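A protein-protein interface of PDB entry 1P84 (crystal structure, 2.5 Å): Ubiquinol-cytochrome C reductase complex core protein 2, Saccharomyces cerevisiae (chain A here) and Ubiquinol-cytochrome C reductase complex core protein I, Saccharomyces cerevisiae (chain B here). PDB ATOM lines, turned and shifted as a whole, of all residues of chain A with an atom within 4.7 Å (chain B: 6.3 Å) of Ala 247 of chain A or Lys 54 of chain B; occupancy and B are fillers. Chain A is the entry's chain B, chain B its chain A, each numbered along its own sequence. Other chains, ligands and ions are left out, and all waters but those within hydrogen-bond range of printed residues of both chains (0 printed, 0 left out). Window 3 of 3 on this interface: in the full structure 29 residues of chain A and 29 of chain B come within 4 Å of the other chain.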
ATOM      1  N   SER A 246     -27.409  25.962 -24.811  1.00  0.00           N
ATOM      2  CA  SER A 246     -26.141  26.291 -24.167  1.00  0.00           C
ATOM      3  C   SER A 246     -24.909  25.915 -24.980  1.00  0.00           C
ATOM      4  O   SER A 246     -24.998  25.221 -25.997  1.00  0.00           O
ATOM      5  CB  SER A 246     -26.053  25.644 -22.780  1.00  0.00           C
ATOM      6  OG  SER A 246     -26.103  24.232 -22.866  1.00  0.00           O
ATOM      7  N   ALA A 247     -23.756  26.367 -24.493  1.00  0.00           N
ATOM      8  CA  ALA A 247     -22.478  26.114 -25.141  1.00  0.00           C
ATOM      9  C   ALA A 247     -22.034  24.652 -25.061  1.00  0.00           C
ATOM     10  O   ALA A 247     -21.231  24.194 -25.879  1.00  0.00           O
ATOM     11  CB  ALA A 247     -21.422  27.017 -24.543  1.00  0.00           C
ATOM     12  N   LEU A 248     -22.564  23.922 -24.083  1.00  0.00           N
ATOM     13  CA  LEU A 248     -22.219  22.517 -23.891  1.00  0.00           C
ATOM     14  C   LEU A 248     -22.721  21.627 -25.020  1.00  0.00           C
ATOM     15  O   LEU A 248     -21.991  20.762 -25.499  1.00  0.00           O
ATOM     16  CB  LEU A 248     -22.730  22.026 -22.538  1.00  0.00           C
ATOM     17  CG  LEU A 248     -22.181  22.835 -21.360  1.00  0.00           C
ATOM     18  CD1 LEU A 248     -22.636  22.237 -20.047  1.00  0.00           C
ATOM     19  CD2 LEU A 248     -20.666  22.875 -21.421  1.00  0.00           C
ATOM     20  N   SER A 249     -23.964  21.830 -25.443  1.00  0.00           N
ATOM     21  CA  SER A 249     -24.511  21.046 -26.540  1.00  0.00           C
ATOM     22  C   SER A 249     -23.934  21.573 -27.842  1.00  0.00           C
ATOM     23  O   SER A 249     -23.725  22.779 -27.997  1.00  0.00           O
ATOM     24  CB  SER A 249     -26.033  21.139 -26.586  1.00  0.00           C
ATOM     25  OG  SER A 249     -26.537  20.429 -27.705  1.00  0.00           O
ATOM     26  N   GLU A 250     -23.662  20.662 -28.767  1.00  0.00           N
ATOM     27  CA  GLU A 250     -23.106  21.034 -30.060  1.00  0.00           C
ATOM     28  C   GLU A 250     -24.188  21.594 -30.971  1.00  0.00           C
ATOM     29  O   GLU A 250     -23.927  22.480 -31.790  1.00  0.00           O
ATOM     30  CB  GLU A 250     -22.455  19.826 -30.732  1.00  0.00           C
ATOM     31  CG  GLU A 250     -21.300  19.216 -29.959  1.00  0.00           C
ATOM     32  CD  GLU A 250     -20.612  18.103 -30.734  1.00  0.00           C
ATOM     33  OE1 GLU A 250     -21.283  17.095 -31.062  1.00  0.00           O
ATOM     34  OE2 GLU A 250     -19.404  18.244 -31.025  1.00  0.00           O
ATOM     35  N   SER A 252     -26.705  23.560 -30.293  1.00  0.00           N
ATOM     36  CA  SER A 252     -27.367  24.752 -29.766  1.00  0.00           C
ATOM     37  C   SER A 252     -27.485  25.807 -30.866  1.00  0.00           C
ATOM     38  O   SER A 252     -28.368  26.665 -30.828  1.00  0.00           O
ATOM     39  CB  SER A 252     -26.599  25.324 -28.570  1.00  0.00           C
ATOM     40  OG  SER A 252     -25.316  25.794 -28.945  1.00  0.00           O
ATOM     41  N   GLY A 253     -26.580  25.733 -31.838  1.00  0.00           N
ATOM     42  CA  GLY A 253     -26.588  26.666 -32.948  1.00  0.00           C
ATOM     43  C   GLY A 253     -27.532  26.220 -34.052  1.00  0.00           C
ATOM     44  O   GLY A 253     -27.658  26.894 -35.077  1.00  0.00           O
ATOM     45  N   ASN B  49     -18.142  39.518 -28.501  1.00  0.00           N
ATOM     46  CA  ASN B  49     -18.566  38.304 -29.187  1.00  0.00           C
ATOM     47  C   ASN B  49     -17.651  37.088 -29.044  1.00  0.00           C
ATOM     48  O   ASN B  49     -18.125  35.949 -29.115  1.00  0.00           O
ATOM     49  CB  ASN B  49     -18.864  38.594 -30.659  1.00  0.00           C
ATOM     50  CG  ASN B  49     -20.209  39.260 -30.856  1.00  0.00           C
ATOM     51  OD1 ASN B  49     -21.233  38.589 -30.996  1.00  0.00           O
ATOM     52  ND2 ASN B  49     -20.217  40.587 -30.866  1.00  0.00           N
ATOM     53  N   ILE B  50     -16.348  37.309 -28.884  1.00  0.00           N
ATOM     54  CA  ILE B  50     -15.444  36.173 -28.705  1.00  0.00           C
ATOM     55  C   ILE B  50     -15.476  35.744 -27.233  1.00  0.00           C
ATOM     56  O   ILE B  50     -15.442  34.552 -26.919  1.00  0.00           O
ATOM     57  CB  ILE B  50     -13.979  36.457 -29.173  1.00  0.00           C
ATOM     58  CG1 ILE B  50     -13.354  37.604 -28.383  1.00  0.00           C
ATOM     59  CG2 ILE B  50     -13.936  36.743 -30.669  1.00  0.00           C
ATOM     60  CD1 ILE B  50     -11.948  37.890 -28.803  1.00  0.00           C
ATOM     61  N   LEU B  52     -17.875  35.662 -25.507  1.00  0.00           N
ATOM     62  CA  LEU B  52     -19.101  34.879 -25.379  1.00  0.00           C
ATOM     63  C   LEU B  52     -19.116  33.712 -26.363  1.00  0.00           C
ATOM     64  O   LEU B  52     -20.125  33.009 -26.482  1.00  0.00           O
ATOM     65  CB  LEU B  52     -20.328  35.756 -25.654  1.00  0.00           C
ATOM     66  CG  LEU B  52     -20.611  36.987 -24.791  1.00  0.00           C
ATOM     67  CD1 LEU B  52     -21.924  37.616 -25.234  1.00  0.00           C
ATOM     68  CD2 LEU B  52     -20.685  36.603 -23.326  1.00  0.00           C
ATOM     69  N   SER B  53     -18.005  33.509 -27.068  1.00  0.00           N
ATOM     70  CA  SER B  53     -17.904  32.444 -28.066  1.00  0.00           C
ATOM     71  C   SER B  53     -18.153  31.052 -27.512  1.00  0.00           C
ATOM     72  O   SER B  53     -17.909  30.789 -26.337  1.00  0.00           O
ATOM     73  CB  SER B  53     -16.547  32.480 -28.766  1.00  0.00           C
ATOM     74  OG  SER B  53     -16.505  31.539 -29.826  1.00  0.00           O
ATOM     75  N   LYS B  54     -18.599  30.158 -28.393  1.00  0.00           N
ATOM     76  CA  LYS B  54     -18.913  28.777 -28.042  1.00  0.00           C
ATOM     77  C   LYS B  54     -17.834  28.082 -27.215  1.00  0.00           C
ATOM     78  O   LYS B  54     -18.146  27.362 -26.267  1.00  0.00           O
ATOM     79  CB  LYS B  54     -19.231  27.970 -29.305  1.00  0.00           C
ATOM     80  CG  LYS B  54     -19.708  26.552 -29.034  1.00  0.00           C
ATOM     81  CD  LYS B  54     -20.425  25.960 -30.238  1.00  0.00           C
ATOM     82  CE  LYS B  54     -21.761  26.657 -30.498  1.00  0.00           C
ATOM     83  NZ  LYS B  54     -22.540  26.005 -31.591  1.00  0.00           N
ATOM     84  N   GLU B  55     -16.569  28.313 -27.561  1.00  0.00           N
ATOM     85  CA  GLU B  55     -15.457  27.710 -26.829  1.00  0.00           C
ATOM     86  C   GLU B  55     -15.414  28.192 -25.383  1.00  0.00           C
ATOM     87  O   GLU B  55     -15.634  27.416 -24.455  1.00  0.00           O
ATOM     88  CB  GLU B  55     -14.117  28.038 -27.492  1.00  0.00           C
ATOM     89  CG  GLU B  55     -13.819  27.281 -28.773  1.00  0.00           C
ATOM     90  CD  GLU B  55     -12.360  27.419 -29.194  1.00  0.00           C
ATOM     91  OE1 GLU B  55     -11.889  28.564 -29.382  1.00  0.00           O
ATOM     92  OE2 GLU B  55     -11.677  26.380 -29.325  1.00  0.00           O
ATOM     93  N   ASN B  56     -15.146  29.483 -25.210  1.00  0.00           N
ATOM     94  CA  ASN B  56     -15.046  30.103 -23.894  1.00  0.00           C
ATOM     95  C   ASN B  56     -16.310  29.943 -23.062  1.00  0.00           C
ATOM     96  O   ASN B  56     -16.239  29.761 -21.849  1.00  0.00           O
ATOM     97  CB  ASN B  56     -14.715  31.590 -24.049  1.00  0.00           C
ATOM     98  CG  ASN B  56     -14.245  32.224 -22.756  1.00  0.00           C
ATOM     99  OD1 ASN B  56     -13.379  31.686 -22.069  1.00  0.00           O
ATOM    100  ND2 ASN B  56     -14.804  33.379 -22.427  1.00  0.00           N
ATOM    101  N   SER B  57     -17.462  29.991 -23.722  1.00  0.00           N
ATOM    102  CA  SER B  57     -18.748  29.871 -23.039  1.00  0.00           C
ATOM    103  C   SER B  57     -19.010  28.456 -22.521  1.00  0.00           C
ATOM    104  O   SER B  57     -19.678  28.281 -21.502  1.00  0.00           O
ATOM    105  CB  SER B  57     -19.888  30.329 -23.962  1.00  0.00           C
ATOM    106  OG  SER B  57     -21.050  30.685 -23.229  1.00  0.00           O
ATOM    107  N   ALA B  58     -18.486  27.453 -23.223  1.00  0.00           N
ATOM    108  CA  ALA B  58     -18.663  26.056 -22.822  1.00  0.00           C
ATOM    109  C   ALA B  58     -17.837  25.716 -21.581  1.00  0.00           C
ATOM    110  O   ALA B  58     -18.216  24.847 -20.791  1.00  0.00           O
ATOM    111  CB  ALA B  58     -18.299  25.123 -23.971  1.00  0.00           C
ATOM    112  N   VAL B  59     -16.715  26.412 -21.415  1.00  0.00           N
ATOM    113  CA  VAL B  59     -15.825  26.200 -20.278  1.00  0.00           C
ATOM    114  C   VAL B  59     -16.486  26.624 -18.971  1.00  0.00           C
ATOM    115  O   VAL B  59     -16.446  25.886 -17.989  1.00  0.00           O
ATOM    116  CB  VAL B  59     -14.494  26.969 -20.453  1.00  0.00           C
ATOM    117  CG1 VAL B  59     -13.610  26.785 -19.236  1.00  0.00           C
ATOM    118  CG2 VAL B  59     -13.772  26.489 -21.700  1.00  0.00           C
ATOM    119  N   ALA B  61     -19.699  27.059 -18.561  1.00  0.00           N
ATOM    120  CA  ALA B  61     -20.979  26.362 -18.449  1.00  0.00           C
ATOM    121  C   ALA B  61     -20.834  25.049 -17.690  1.00  0.00           C
ATOM    122  O   ALA B  61     -21.715  24.679 -16.914  1.00  0.00           O
ATOM    123  CB  ALA B  61     -21.574  26.120 -19.825  1.00  0.00           C
ATOM    124  N   ASN B 110     -11.351  30.503 -34.513  1.00  0.00           N
ATOM    125  CA  ASN B 110     -12.374  31.072 -33.644  1.00  0.00           C
ATOM    126  C   ASN B 110     -12.753  32.465 -34.150  1.00  0.00           C
ATOM    127  O   ASN B 110     -13.932  32.765 -34.350  1.00  0.00           O
ATOM    128  CB  ASN B 110     -11.843  31.154 -32.205  1.00  0.00           C
ATOM    129  CG  ASN B 110     -12.947  31.337 -31.178  1.00  0.00           C
ATOM    130  OD1 ASN B 110     -13.955  30.626 -31.199  1.00  0.00           O
ATOM    131  ND2 ASN B 110     -12.752  32.279 -30.259  1.00  0.00           N
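Printed residues of chain A that touch a printed residue of chain B: Ala 247, Leu 248, Glu 250 and Ser 252. Of the 12 printed residues of chain B, 4 touch a printed residue of chain A. Printed residues of chain B that touch a printed residue of chain A: Lys 54, Ser 57, Ala 58 and Ala 61. Hydrophobic or aromatic side chains of chain B within 4 Å of the printed part of chain A: Ala 58 and Ala 61.
Of chain B, only Lys 54 (3.7 Å), Ser 57 (3.5 Å) and Ala 58 (3.2 Å) come within 4 Å of Ala 247 of chain A. Lys 54 of chain B touches just these residues of chain A: Ala 247 (3.7 Å), Glu 250 (3.8 Å) and Ser 252 (3.8 Å). Printed residues of chain A within 4 Å of Ala 61 of chain B: Leu 248. Of the printed residues of chain B, Ser 252 of chain A touches Lys 54 (3.8 Å). Asn 110 of chain B touches none of the printed residues of chain A. Ile 50 of chain B touches none of the printed residues of chain A. The nearest residue of chain B that does not touch Ala 247 of chain A is Ala 61 of chain B (4.8 Å). The nearest residue of chain A that does not touch Lys 54 of chain B is Gly 253 of chain A (4.1 Å). The nearest printed residue of chain B that does not touch Glu 250 of chain A is Ala 58 of chain B (8.5 Å).
O of Ser 246 of chain A is in hydrogen-bond range of OG of Ser 252 of chain A (3.0 Å).
Among the printed residues, pairs that only touch across the chains: Ala 247 of chain A with Lys 54 of chain B (3.7 Å), Ala 247 of chain A with Ser 57 of chain B (3.5 Å), Ala 247 of chain A with Ala 58 of chain B (3.2 Å), Leu 248 of chain A with Ala 58 of chain B (3.2 Å), Leu 248 of chain A with Ala 61 of chain B (3.7 Å), Glu 250 of chain A with Lys 54 of chain B (3.8 Å) and Ser 252 of chain A with Lys 54 of chain B (3.8 Å).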
